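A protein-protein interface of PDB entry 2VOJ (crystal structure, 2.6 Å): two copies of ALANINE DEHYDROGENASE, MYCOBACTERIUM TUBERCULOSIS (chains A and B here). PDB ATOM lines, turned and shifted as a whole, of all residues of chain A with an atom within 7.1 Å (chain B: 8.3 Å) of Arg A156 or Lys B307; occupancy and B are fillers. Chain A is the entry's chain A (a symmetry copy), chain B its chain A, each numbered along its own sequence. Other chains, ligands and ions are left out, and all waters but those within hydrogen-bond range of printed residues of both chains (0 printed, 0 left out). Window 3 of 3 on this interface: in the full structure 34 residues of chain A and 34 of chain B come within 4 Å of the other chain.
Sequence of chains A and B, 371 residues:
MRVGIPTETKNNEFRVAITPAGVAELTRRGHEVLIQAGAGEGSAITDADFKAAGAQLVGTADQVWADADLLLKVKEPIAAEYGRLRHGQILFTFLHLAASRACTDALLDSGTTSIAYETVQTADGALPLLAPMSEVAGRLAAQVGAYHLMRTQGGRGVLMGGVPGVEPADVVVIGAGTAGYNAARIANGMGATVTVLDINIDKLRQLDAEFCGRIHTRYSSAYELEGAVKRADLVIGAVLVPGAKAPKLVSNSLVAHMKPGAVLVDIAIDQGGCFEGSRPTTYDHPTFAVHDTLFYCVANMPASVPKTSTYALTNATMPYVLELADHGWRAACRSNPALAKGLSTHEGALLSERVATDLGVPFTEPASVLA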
ATOM      1  N   HIS A 148      31.577  -3.064 -12.977  1.00  0.00           N
ATOM      2  CA  HIS A 148      31.853  -1.739 -12.400  1.00  0.00           C
ATOM      3  C   HIS A 148      32.064  -0.660 -13.450  1.00  0.00           C
ATOM      4  O   HIS A 148      32.226   0.500 -13.116  1.00  0.00           O
ATOM      5  CB  HIS A 148      33.021  -1.786 -11.413  1.00  0.00           C
ATOM      6  CG  HIS A 148      32.731  -2.642 -10.223  1.00  0.00           C
ATOM      7  ND1 HIS A 148      32.158  -2.142  -9.072  1.00  0.00           N
ATOM      8  CD2 HIS A 148      32.836  -3.979 -10.041  1.00  0.00           C
ATOM      9  CE1 HIS A 148      31.957  -3.126  -8.215  1.00  0.00           C
ATOM     10  NE2 HIS A 148      32.349  -4.254  -8.781  1.00  0.00           N
ATOM     11  N   LEU A 149      32.029  -1.033 -14.722  1.00  0.00           N
ATOM     12  CA  LEU A 149      32.050  -0.047 -15.781  1.00  0.00           C
ATOM     13  C   LEU A 149      30.655   0.576 -16.008  1.00  0.00           C
ATOM     14  O   LEU A 149      30.537   1.601 -16.668  1.00  0.00           O
ATOM     15  CB  LEU A 149      32.607  -0.689 -17.058  1.00  0.00           C
ATOM     16  CG  LEU A 149      33.772  -0.072 -17.810  1.00  0.00           C
ATOM     17  CD1 LEU A 149      34.599   0.865 -16.982  1.00  0.00           C
ATOM     18  CD2 LEU A 149      34.626  -1.156 -18.390  1.00  0.00           C
ATOM     19  N   MET A 150      29.613  -0.039 -15.456  1.00  0.00           N
ATOM     20  CA  MET A 150      28.254   0.538 -15.507  1.00  0.00           C
ATOM     21  C   MET A 150      28.159   1.828 -14.679  1.00  0.00           C
ATOM     22  O   MET A 150      28.717   1.900 -13.582  1.00  0.00           O
ATOM     23  CB  MET A 150      27.213  -0.474 -15.017  1.00  0.00           C
ATOM     24  CG  MET A 150      27.306  -1.834 -15.640  1.00  0.00           C
ATOM     25  SD  MET A 150      25.884  -2.864 -15.341  1.00  0.00           S
ATOM     26  CE  MET A 150      25.970  -3.078 -13.594  1.00  0.00           C
ATOM     27  N   ARG A 151      27.448   2.833 -15.192  1.00  0.00           N
ATOM     28  CA  ARG A 151      27.356   4.136 -14.496  1.00  0.00           C
ATOM     29  C   ARG A 151      26.721   3.970 -13.121  1.00  0.00           C
ATOM     30  O   ARG A 151      27.081   4.610 -12.159  1.00  0.00           O
ATOM     31  CB  ARG A 151      26.629   5.216 -15.320  1.00  0.00           C
ATOM     32  CG  ARG A 151      27.274   6.596 -15.115  1.00  0.00           C
ATOM     33  CD  ARG A 151      26.271   7.727 -15.154  1.00  0.00           C
ATOM     34  NE  ARG A 151      26.661   8.809 -14.256  1.00  0.00           N
ATOM     35  CZ  ARG A 151      26.391   8.855 -12.942  1.00  0.00           C
ATOM     36  NH1 ARG A 151      25.706   7.882 -12.340  1.00  0.00           N
ATOM     37  NH2 ARG A 151      26.812   9.883 -12.214  1.00  0.00           N
ATOM     38  N   GLY A 154      29.264   3.593 -10.502  1.00  0.00           N
ATOM     39  CA  GLY A 154      30.335   4.583 -10.482  1.00  0.00           C
ATOM     40  C   GLY A 154      31.271   4.603 -11.684  1.00  0.00           C
ATOM     41  O   GLY A 154      32.058   5.527 -11.805  1.00  0.00           O
ATOM     42  N   GLY A 155      31.201   3.619 -12.588  1.00  0.00           N
ATOM     43  CA  GLY A 155      32.050   3.615 -13.797  1.00  0.00           C
ATOM     44  C   GLY A 155      31.602   4.569 -14.897  1.00  0.00           C
ATOM     45  O   GLY A 155      30.576   5.234 -14.766  1.00  0.00           O
ATOM     46  N   ARG A 156      32.342   4.623 -16.005  1.00  0.00           N
ATOM     47  CA  ARG A 156      31.973   5.566 -17.066  1.00  0.00           C
ATOM     48  C   ARG A 156      30.745   5.279 -17.902  1.00  0.00           C
ATOM     49  O   ARG A 156      30.376   6.123 -18.702  1.00  0.00           O
ATOM     50  CB  ARG A 156      33.123   5.916 -17.996  1.00  0.00           C
ATOM     51  CG  ARG A 156      34.142   4.874 -18.206  1.00  0.00           C
ATOM     52  CD  ARG A 156      35.065   5.348 -19.331  1.00  0.00           C
ATOM     53  NE  ARG A 156      35.115   6.801 -19.395  1.00  0.00           N
ATOM     54  CZ  ARG A 156      34.938   7.521 -20.490  1.00  0.00           C
ATOM     55  NH1 ARG A 156      34.708   6.923 -21.642  1.00  0.00           N
ATOM     56  NH2 ARG A 156      35.013   8.844 -20.419  1.00  0.00           N
ATOM     57  N   GLY A 157      30.145   4.104 -17.737  1.00  0.00           N
ATOM     58  CA  GLY A 157      28.953   3.709 -18.477  1.00  0.00           C
ATOM     59  C   GLY A 157      29.160   3.269 -19.917  1.00  0.00           C
ATOM     60  O   GLY A 157      28.398   3.676 -20.773  1.00  0.00           O
ATOM     61  N   VAL A 158      30.185   2.445 -20.176  1.00  0.00           N
ATOM     62  CA  VAL A 158      30.389   1.814 -21.480  1.00  0.00           C
ATOM     63  C   VAL A 158      30.202   0.327 -21.329  1.00  0.00           C
ATOM     64  O   VAL A 158      30.642  -0.258 -20.342  1.00  0.00           O
ATOM     65  CB  VAL A 158      31.812   2.066 -22.081  1.00  0.00           C
ATOM     66  CG1 VAL A 158      32.055   3.556 -22.317  1.00  0.00           C
ATOM     67  CG2 VAL A 158      32.896   1.517 -21.156  1.00  0.00           C
ATOM     68  N   LEU A 159      29.554  -0.279 -22.317  1.00  0.00           N
ATOM     69  CA  LEU A 159      29.420  -1.725 -22.391  1.00  0.00           C
ATOM     70  C   LEU A 159      30.739  -2.335 -22.893  1.00  0.00           C
ATOM     71  O   LEU A 159      31.294  -1.855 -23.880  1.00  0.00           O
ATOM     72  CB  LEU A 159      28.277  -2.040 -23.337  1.00  0.00           C
ATOM     73  CG  LEU A 159      27.832  -3.465 -23.581  1.00  0.00           C
ATOM     74  CD1 LEU A 159      27.434  -4.140 -22.294  1.00  0.00           C
ATOM     75  CD2 LEU A 159      26.670  -3.358 -24.512  1.00  0.00           C
ATOM     76  N   VAL A 166      28.970   1.185 -32.564  1.00  0.00           N
ATOM     77  CA  VAL A 166      29.464   1.919 -31.426  1.00  0.00           C
ATOM     78  C   VAL A 166      30.709   1.207 -30.848  1.00  0.00           C
ATOM     79  O   VAL A 166      30.716  -0.017 -30.709  1.00  0.00           O
ATOM     80  CB  VAL A 166      28.351   2.029 -30.312  1.00  0.00           C
ATOM     81  CG1 VAL A 166      28.869   2.749 -29.069  1.00  0.00           C
ATOM     82  CG2 VAL A 166      27.094   2.702 -30.827  1.00  0.00           C
ATOM     83  N   GLU A 167      31.731   1.974 -30.463  1.00  0.00           N
ATOM     84  CA  GLU A 167      32.998   1.394 -30.006  1.00  0.00           C
ATOM     85  C   GLU A 167      32.923   0.570 -28.694  1.00  0.00           C
ATOM     86  O   GLU A 167      32.199   0.924 -27.751  1.00  0.00           O
ATOM     87  CB  GLU A 167      34.079   2.486 -29.882  1.00  0.00           C
ATOM     88  CG  GLU A 167      33.855   3.480 -28.721  1.00  0.00           C
ATOM     89  CD  GLU A 167      35.097   4.351 -28.396  1.00  0.00           C
ATOM     90  OE1 GLU A 167      36.194   4.103 -28.988  1.00  0.00           O
ATOM     91  OE2 GLU A 167      34.980   5.273 -27.526  1.00  0.00           O
ATOM     92  N   ALA A 232      42.683   3.766 -21.534  1.00  0.00           N
ATOM     93  CA  ALA A 232      41.900   2.612 -21.129  1.00  0.00           C
ATOM     94  C   ALA A 232      40.640   2.959 -20.341  1.00  0.00           C
ATOM     95  O   ALA A 232      40.644   3.897 -19.568  1.00  0.00           O
ATOM     96  CB  ALA A 232      42.777   1.639 -20.319  1.00  0.00           C
ATOM     97  N   ASP A 233      39.585   2.170 -20.528  1.00  0.00           N
ATOM     98  CA  ASP A 233      38.418   2.159 -19.644  1.00  0.00           C
ATOM     99  C   ASP A 233      38.594   1.209 -18.461  1.00  0.00           C
ATOM    100  O   ASP A 233      38.061   1.453 -17.383  1.00  0.00           O
ATOM    101  CB  ASP A 233      37.170   1.745 -20.405  1.00  0.00           C
ATOM    102  CG  ASP A 233      36.926   2.603 -21.608  1.00  0.00           C
ATOM    103  OD1 ASP A 233      36.740   3.808 -21.443  1.00  0.00           O
ATOM    104  OD2 ASP A 233      36.930   2.090 -22.731  1.00  0.00           O
ATOM    105  N   LEU A 234      39.328   0.121 -18.680  1.00  0.00           N
ATOM    106  CA  LEU A 234      39.511  -0.928 -17.673  1.00  0.00           C
ATOM    107  C   LEU A 234      40.977  -1.319 -17.684  1.00  0.00           C
ATOM    108  O   LEU A 234      41.505  -1.674 -18.737  1.00  0.00           O
ATOM    109  CB  LEU A 234      38.690  -2.157 -18.036  1.00  0.00           C
ATOM    110  CG  LEU A 234      38.173  -3.169 -17.009  1.00  0.00           C
ATOM    111  CD1 LEU A 234      38.187  -4.554 -17.608  1.00  0.00           C
ATOM    112  CD2 LEU A 234      38.833  -3.164 -15.650  1.00  0.00           C
ATOM    113  N   LYS A 259      40.693   8.704 -18.035  1.00  0.00           N
ATOM    114  CA  LYS A 259      39.302   9.065 -18.233  1.00  0.00           C
ATOM    115  C   LYS A 259      38.527   8.910 -16.919  1.00  0.00           C
ATOM    116  O   LYS A 259      38.710   7.933 -16.199  1.00  0.00           O
ATOM    117  CB  LYS A 259      38.657   8.212 -19.322  1.00  0.00           C
ATOM    118  CG  LYS A 259      39.498   7.981 -20.547  1.00  0.00           C
ATOM    119  CD  LYS A 259      38.586   7.755 -21.714  1.00  0.00           C
ATOM    120  CE  LYS A 259      39.127   6.728 -22.692  1.00  0.00           C
ATOM    121  NZ  LYS A 259      38.581   5.387 -22.411  1.00  0.00           N
ATOM    122  N   PRO A 260      37.684   9.893 -16.585  1.00  0.00           N
ATOM    123  CA  PRO A 260      36.790   9.754 -15.412  1.00  0.00           C
ATOM    124  C   PRO A 260      35.921   8.484 -15.444  1.00  0.00           C
ATOM    125  O   PRO A 260      35.398   8.132 -16.504  1.00  0.00           O
ATOM    126  CB  PRO A 260      35.916  11.010 -15.488  1.00  0.00           C
ATOM    127  CG  PRO A 260      36.708  11.970 -16.305  1.00  0.00           C
ATOM    128  CD  PRO A 260      37.567  11.204 -17.244  1.00  0.00           C
ATOM    129  N   GLY A 261      35.793   7.793 -14.307  1.00  0.00           N
ATOM    130  CA  GLY A 261      35.016   6.539 -14.238  1.00  0.00           C
ATOM    131  C   GLY A 261      35.716   5.251 -14.716  1.00  0.00           C
ATOM    132  O   GLY A 261      35.128   4.168 -14.696  1.00  0.00           O
ATOM    133  N   ALA A 262      36.968   5.362 -15.146  1.00  0.00           N
ATOM    134  CA  ALA A 262      37.779   4.199 -15.453  1.00  0.00           C
ATOM    135  C   ALA A 262      37.873   3.249 -14.237  1.00  0.00           C
ATOM    136  O   ALA A 262      37.762   3.677 -13.079  1.00  0.00           O
ATOM    137  CB  ALA A 262      39.153   4.633 -15.907  1.00  0.00           C
ATOM    138  N   VAL A 263      38.015   1.952 -14.501  1.00  0.00           N
ATOM    139  CA  VAL A 263      38.190   1.027 -13.406  1.00  0.00           C
ATOM    140  C   VAL A 263      39.497   0.284 -13.462  1.00  0.00           C
ATOM    141  O   VAL A 263      39.962  -0.088 -14.535  1.00  0.00           O
ATOM    142  CB  VAL A 263      36.918   0.154 -13.033  1.00  0.00           C
ATOM    143  CG1 VAL A 263      35.765   0.392 -13.914  1.00  0.00           C
ATOM    144  CG2 VAL A 263      37.228  -1.301 -12.878  1.00  0.00           C
ATOM    145  N   LEU A 294      37.939   4.321 -10.276  1.00  0.00           N
ATOM    146  CA  LEU A 294      37.431   3.395  -9.292  1.00  0.00           C
ATOM    147  C   LEU A 294      38.396   2.214  -9.216  1.00  0.00           C
ATOM    148  O   LEU A 294      38.720   1.616 -10.247  1.00  0.00           O
ATOM    149  CB  LEU A 294      36.076   2.943  -9.751  1.00  0.00           C
ATOM    150  CG  LEU A 294      34.983   2.510  -8.822  1.00  0.00           C
ATOM    151  CD1 LEU A 294      34.526   3.648  -7.949  1.00  0.00           C
ATOM    152  CD2 LEU A 294      33.864   2.067  -9.722  1.00  0.00           C
ATOM    153  N   PHE B  14      19.736   7.122 -17.354  1.00  0.00           N
ATOM    154  CA  PHE B  14      20.789   8.072 -17.698  1.00  0.00           C
ATOM    155  C   PHE B  14      20.812   8.411 -19.174  1.00  0.00           C
ATOM    156  O   PHE B  14      21.580   9.284 -19.603  1.00  0.00           O
ATOM    157  CB  PHE B  14      22.161   7.548 -17.269  1.00  0.00           C
ATOM    158  CG  PHE B  14      22.310   7.387 -15.786  1.00  0.00           C
ATOM    159  CD1 PHE B  14      22.577   8.488 -14.972  1.00  0.00           C
ATOM    160  CD2 PHE B  14      22.162   6.146 -15.193  1.00  0.00           C
ATOM    161  CE1 PHE B  14      22.703   8.346 -13.582  1.00  0.00           C
ATOM    162  CE2 PHE B  14      22.295   6.000 -13.812  1.00  0.00           C
ATOM    163  CZ  PHE B  14      22.565   7.103 -13.011  1.00  0.00           C
ATOM    164  N   ARG B  15      19.991   7.715 -19.964  1.00  0.00           N
ATOM    165  CA  ARG B  15      19.905   8.020 -21.386  1.00  0.00           C
ATOM    166  C   ARG B  15      19.195   9.337 -21.665  1.00  0.00           C
ATOM    167  O   ARG B  15      18.501   9.876 -20.810  1.00  0.00           O
ATOM    168  CB  ARG B  15      19.236   6.890 -22.173  1.00  0.00           C
ATOM    169  CG  ARG B  15      20.044   5.594 -22.211  1.00  0.00           C
ATOM    170  CD  ARG B  15      19.231   4.431 -22.755  1.00  0.00           C
ATOM    171  NE  ARG B  15      18.222   4.015 -21.792  1.00  0.00           N
ATOM    172  CZ  ARG B  15      17.335   3.048 -21.995  1.00  0.00           C
ATOM    173  NH1 ARG B  15      17.310   2.412 -23.149  1.00  0.00           N
ATOM    174  NH2 ARG B  15      16.446   2.744 -21.054  1.00  0.00           N
ATOM    175  N   GLY B  40      20.959  15.874 -20.808  1.00  0.00           N
ATOM    176  CA  GLY B  40      22.039  15.064 -21.322  1.00  0.00           C
ATOM    177  C   GLY B  40      23.123  14.725 -20.313  1.00  0.00           C
ATOM    178  O   GLY B  40      24.114  14.094 -20.660  1.00  0.00           O
ATOM    179  N   GLU B  41      22.962  15.146 -19.068  1.00  0.00           N
ATOM    180  CA  GLU B  41      24.061  14.986 -18.118  1.00  0.00           C
ATOM    181  C   GLU B  41      24.403  13.532 -17.784  1.00  0.00           C
ATOM    182  O   GLU B  41      25.577  13.197 -17.678  1.00  0.00           O
ATOM    183  CB  GLU B  41      23.903  15.877 -16.884  1.00  0.00           C
ATOM    184  CG  GLU B  41      24.614  17.239 -17.093  1.00  0.00           C
ATOM    185  CD  GLU B  41      24.108  18.347 -16.161  1.00  0.00           C
ATOM    186  OE1 GLU B  41      23.861  18.075 -14.956  1.00  0.00           O
ATOM    187  OE2 GLU B  41      23.961  19.500 -16.638  1.00  0.00           O
ATOM    188  N   GLY B  42      23.395  12.667 -17.681  1.00  0.00           N
ATOM    189  CA  GLY B  42      23.625  11.229 -17.477  1.00  0.00           C
ATOM    190  C   GLY B  42      24.498  10.577 -18.553  1.00  0.00           C
ATOM    191  O   GLY B  42      25.258   9.639 -18.269  1.00  0.00           O
ATOM    192  N   SER B  43      24.383  11.071 -19.788  1.00  0.00           N
ATOM    193  CA  SER B  43      25.160  10.571 -20.913  1.00  0.00           C
ATOM    194  C   SER B  43      26.348  11.465 -21.226  1.00  0.00           C
ATOM    195  O   SER B  43      26.890  11.373 -22.304  1.00  0.00           O
ATOM    196  CB  SER B  43      24.300  10.431 -22.182  1.00  0.00           C
ATOM    197  OG  SER B  43      23.157   9.635 -21.983  1.00  0.00           O
ATOM    198  N   ALA B  44      26.742  12.333 -20.296  1.00  0.00           N
ATOM    199  CA  ALA B  44      27.917  13.209 -20.459  1.00  0.00           C
ATOM    200  C   ALA B  44      27.788  14.179 -21.623  1.00  0.00           C
ATOM    201  O   ALA B  44      28.771  14.508 -22.278  1.00  0.00           O
ATOM    202  CB  ALA B  44      29.223  12.406 -20.562  1.00  0.00           C
ATOM    203  N   ILE B  45      26.564  14.629 -21.885  1.00  0.00           N
ATOM    204  CA  ILE B  45      26.345  15.682 -22.861  1.00  0.00           C
ATOM    205  C   ILE B  45      25.914  16.939 -22.119  1.00  0.00           C
ATOM    206  O   ILE B  45      24.857  16.971 -21.486  1.00  0.00           O
ATOM    207  CB  ILE B  45      25.307  15.270 -23.892  1.00  0.00           C
ATOM    208  CG1 ILE B  45      25.755  13.988 -24.616  1.00  0.00           C
ATOM    209  CG2 ILE B  45      25.009  16.424 -24.862  1.00  0.00           C
ATOM    210  CD1 ILE B  45      24.602  13.147 -25.114  1.00  0.00           C
ATOM    211  N   VAL B 136      22.169  -4.106 -26.432  1.00  0.00           N
ATOM    212  CA  VAL B 136      22.723  -3.679 -25.167  1.00  0.00           C
ATOM    213  C   VAL B 136      22.247  -4.585 -24.028  1.00  0.00           C
ATOM    214  O   VAL B 136      23.065  -5.039 -23.229  1.00  0.00           O
ATOM    215  CB  VAL B 136      22.387  -2.178 -24.876  1.00  0.00           C
ATOM    216  CG1 VAL B 136      22.862  -1.769 -23.484  1.00  0.00           C
ATOM    217  CG2 VAL B 136      22.999  -1.261 -25.968  1.00  0.00           C
ATOM    218  N   PRO B 302      19.425  -0.969 -20.404  1.00  0.00           N
ATOM    219  CA  PRO B 302      20.473  -0.184 -21.081  1.00  0.00           C
ATOM    220  C   PRO B 302      20.877   1.147 -20.430  1.00  0.00           C
ATOM    221  O   PRO B 302      21.872   1.753 -20.823  1.00  0.00           O
ATOM    222  CB  PRO B 302      19.875   0.039 -22.490  1.00  0.00           C
ATOM    223  CG  PRO B 302      18.875  -1.083 -22.648  1.00  0.00           C
ATOM    224  CD  PRO B 302      18.266  -1.200 -21.288  1.00  0.00           C
ATOM    225  N   ALA B 303      20.127   1.590 -19.434  1.00  0.00           N
ATOM    226  CA  ALA B 303      20.392   2.884 -18.782  1.00  0.00           C
ATOM    227  C   ALA B 303      21.738   2.958 -18.062  1.00  0.00           C
ATOM    228  O   ALA B 303      22.295   4.045 -17.952  1.00  0.00           O
ATOM    229  CB  ALA B 303      19.242   3.255 -17.830  1.00  0.00           C
ATOM    230  N   SER B 304      22.250   1.816 -17.593  1.00  0.00           N
ATOM    231  CA  SER B 304      23.545   1.782 -16.879  1.00  0.00           C
ATOM    232  C   SER B 304      24.779   1.984 -17.765  1.00  0.00           C
ATOM    233  O   SER B 304      25.864   2.257 -17.263  1.00  0.00           O
ATOM    234  CB  SER B 304      23.703   0.505 -16.052  1.00  0.00           C
ATOM    235  OG  SER B 304      23.632  -0.640 -16.873  1.00  0.00           O
ATOM    236  N   VAL B 305      24.633   1.880 -19.077  1.00  0.00           N
ATOM    237  CA  VAL B 305      25.778   2.099 -19.978  1.00  0.00           C
ATOM    238  C   VAL B 305      25.456   3.182 -21.001  1.00  0.00           C
ATOM    239  O   VAL B 305      25.539   2.946 -22.204  1.00  0.00           O
ATOM    240  CB  VAL B 305      26.249   0.767 -20.689  1.00  0.00           C
ATOM    241  CG1 VAL B 305      26.882  -0.211 -19.678  1.00  0.00           C
ATOM    242  CG2 VAL B 305      25.104   0.101 -21.433  1.00  0.00           C
ATOM    243  N   PRO B 306      25.091   4.384 -20.525  1.00  0.00           N
ATOM    244  CA  PRO B 306      24.525   5.401 -21.424  1.00  0.00           C
ATOM    245  C   PRO B 306      25.499   5.866 -22.505  1.00  0.00           C
ATOM    246  O   PRO B 306      25.084   6.233 -23.616  1.00  0.00           O
ATOM    247  CB  PRO B 306      24.210   6.568 -20.486  1.00  0.00           C
ATOM    248  CG  PRO B 306      25.065   6.339 -19.300  1.00  0.00           C
ATOM    249  CD  PRO B 306      25.190   4.878 -19.142  1.00  0.00           C
ATOM    250  N   LYS B 307      26.783   5.870 -22.188  1.00  0.00           N
ATOM    251  CA  LYS B 307      27.785   6.171 -23.198  1.00  0.00           C
ATOM    252  C   LYS B 307      27.652   5.292 -24.439  1.00  0.00           C
ATOM    253  O   LYS B 307      27.930   5.752 -25.532  1.00  0.00           O
ATOM    254  CB  LYS B 307      29.204   6.064 -22.638  1.00  0.00           C
ATOM    255  CG  LYS B 307      29.939   7.381 -22.577  1.00  0.00           C
ATOM    256  CD  LYS B 307      29.624   8.114 -21.310  1.00  0.00           C
ATOM    257  CE  LYS B 307      30.887   8.750 -20.700  1.00  0.00           C
ATOM    258  NZ  LYS B 307      30.656   8.862 -19.223  1.00  0.00           N
ATOM    259  N   THR B 308      27.253   4.033 -24.264  1.00  0.00           N
ATOM    260  CA  THR B 308      27.019   3.130 -25.356  1.00  0.00           C
ATOM    261  C   THR B 308      25.581   3.300 -25.850  1.00  0.00           C
ATOM    262  O   THR B 308      25.337   3.438 -27.061  1.00  0.00           O
ATOM    263  CB  THR B 308      27.241   1.615 -24.921  1.00  0.00           C
ATOM    264  OG1 THR B 308      28.569   1.422 -24.440  1.00  0.00           O
ATOM    265  CG2 THR B 308      27.000   0.622 -26.069  1.00  0.00           C
ATOM    266  N   SER B 309      24.626   3.253 -24.922  1.00  0.00           N
ATOM    267  CA  SER B 309      23.245   3.051 -25.324  1.00  0.00           C
ATOM    268  C   SER B 309      22.530   4.314 -25.856  1.00  0.00           C
ATOM    269  O   SER B 309      21.741   4.229 -26.784  1.00  0.00           O
ATOM    270  CB  SER B 309      22.466   2.268 -24.262  1.00  0.00           C
ATOM    271  OG  SER B 309      22.243   3.077 -23.147  1.00  0.00           O
ATOM    272  N   THR B 310      22.852   5.480 -25.327  1.00  0.00           N
ATOM    273  CA  THR B 310      22.350   6.723 -25.941  1.00  0.00           C
ATOM    274  C   THR B 310      22.725   6.854 -27.441  1.00  0.00           C
ATOM    275  O   THR B 310      21.878   7.179 -28.284  1.00  0.00           O
ATOM    276  CB  THR B 310      22.842   7.944 -25.173  1.00  0.00           C
ATOM    277  OG1 THR B 310      22.205   7.926 -23.900  1.00  0.00           O
ATOM    278  CG2 THR B 310      22.498   9.234 -25.899  1.00  0.00           C
ATOM    279  N   TYR B 311      23.986   6.598 -27.768  1.00  0.00           N
ATOM    280  CA  TYR B 311      24.369   6.627 -29.165  1.00  0.00           C
ATOM    281  C   TYR B 311      23.764   5.522 -29.990  1.00  0.00           C
ATOM    282  O   TYR B 311      23.335   5.766 -31.098  1.00  0.00           O
ATOM    283  CB  TYR B 311      25.884   6.712 -29.348  1.00  0.00           C
ATOM    284  CG  TYR B 311      26.390   7.983 -28.768  1.00  0.00           C
ATOM    285  CD1 TYR B 311      26.322   9.187 -29.494  1.00  0.00           C
ATOM    286  CD2 TYR B 311      26.868   8.017 -27.453  1.00  0.00           C
ATOM    287  CE1 TYR B 311      26.766  10.403 -28.920  1.00  0.00           C
ATOM    288  CE2 TYR B 311      27.299   9.210 -26.879  1.00  0.00           C
ATOM    289  CZ  TYR B 311      27.245  10.400 -27.611  1.00  0.00           C
ATOM    290  OH  TYR B 311      27.698  11.567 -27.004  1.00  0.00           O
ATOM    291  N   ALA B 312      23.694   4.319 -29.453  1.00  0.00           N
ATOM    292  CA  ALA B 312      23.072   3.232 -30.172  1.00  0.00           C
ATOM    293  C   ALA B 312      21.588   3.523 -30.471  1.00  0.00           C
ATOM    294  O   ALA B 312      21.102   3.209 -31.569  1.00  0.00           O
ATOM    295  CB  ALA B 312      23.244   1.932 -29.424  1.00  0.00           C
ATOM    296  N   LEU B 313      20.879   4.133 -29.523  1.00  0.00           N
ATOM    297  CA  LEU B 313      19.482   4.414 -29.726  1.00  0.00           C
ATOM    298  C   LEU B 313      19.273   5.503 -30.777  1.00  0.00           C
ATOM    299  O   LEU B 313      18.517   5.314 -31.727  1.00  0.00           O
ATOM    300  CB  LEU B 313      18.786   4.804 -28.429  1.00  0.00           C
ATOM    301  CG  LEU B 313      17.283   5.030 -28.611  1.00  0.00           C
ATOM    302  CD1 LEU B 313      16.607   3.736 -28.952  1.00  0.00           C
ATOM    303  CD2 LEU B 313      16.697   5.582 -27.356  1.00  0.00           C
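The side-chain sulfur (SD) of Met A150 is in hydrogen-bond range of the side-chain hydroxyl (OG) of Ser B304, 3.5 Å away.
The backbone NH (N) of Arg A151 sits at hydrogen-bond distance from the backbone carbonyl oxygen (O) of Ser B304 (2.7 Å).
The backbone carbonyl oxygen of Gly A157 lies close to the backbone nitrogen of Pro B306, 3.4 Å away.
N of Lys B307 sits at hydrogen-bond distance from O of Gly A157.
NZ of Lys B307 is in hydrogen-bond range of O of Arg A156, at 2.8 Å.
The backbone carbonyl oxygen (O) of Gly A157 sits close to the backbone carbonyl oxygen (O) of Val B305, 3.3 Å away.
The side-chain hydroxyl of Thr B308 lies within hydrogen-bond range of the backbone NH of Leu A159 (2.9 Å).
The side-chain carboxylate of Asp A233 lies within salt-bridge range of the guanidinium group of Arg A156, at 3.7 Å.
N of Arg A156 is in hydrogen-bond range of O of Gly A261 (3.1 Å).
The guanidinium group of Arg A156 lies within hydrogen-bond range of the backbone carbonyl oxygen of Pro A260, at 3.2 Å.
The side-chain hydroxyl (OG) of Ser B43 lies within hydrogen-bond range of the backbone carbonyl oxygen (O) of Phe B14.
Arg A151 touches Phe B14.
Arg A151 touches Gly B42 (CD to O, 3.8 Å).
Gly A157 touches Ser B304 (CA to O, 3.6 Å).
Gly A157 touches Thr B308 (O to N, 3.7 Å).
Val B305 touches Val A158.
CB of Lys B307 touches CG1 of Val A158, at 3.8 Å.
Val A158 touches Thr B308.
CG1 of Val B305 touches N of Leu A159, at 3.8 Å.
Arg A156 touches one residue of chain B.
Lys B307 touches just these residues of chain A: Arg A156, Gly A157 and Val A158.
No residue of chain B comes within 4 Å of Gly A155.
Of the printed residues of chain B, Met A150 touches Ser B304.
Of the printed residues of chain A, Pro B306 touches Gly A157 (3.4 Å).
Of the printed residues of chain B, Leu A159 touches Val B305 (3.8 Å) and Thr B308 (2.9 Å).
Of the printed residues of chain A, Gly B42 touches Arg A151 (3.8 Å).
Pro B302 touches none of the printed residues of chain A.
Gly A154 touches none of the printed residues of chain B.
The nearest residue of chain A that does not touch Lys B307 is Val A166 (4.7 Å).
The nearest printed residue of chain A that does not touch Pro B306 is Arg A151 (4.1 Å).
Printed residues of chain B that touch a printed residue of chain A: Phe B14, Gly B42, Ser B304, Val B305, Pro B306, Lys B307 and Thr B308.
Hydrophobic or aromatic side chains of chain B within 4 Å of the printed part of chain A: Phe B14, Val B305 and Pro B306.
Of the 21 printed residues of chain A, 6 touch a printed residue of chain B.
Printed residues of chain A that touch a printed residue of chain B: Met A150, Arg A151, Arg A156, Gly A157, Val A158 and Leu A159.
No position is printed for both chains.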
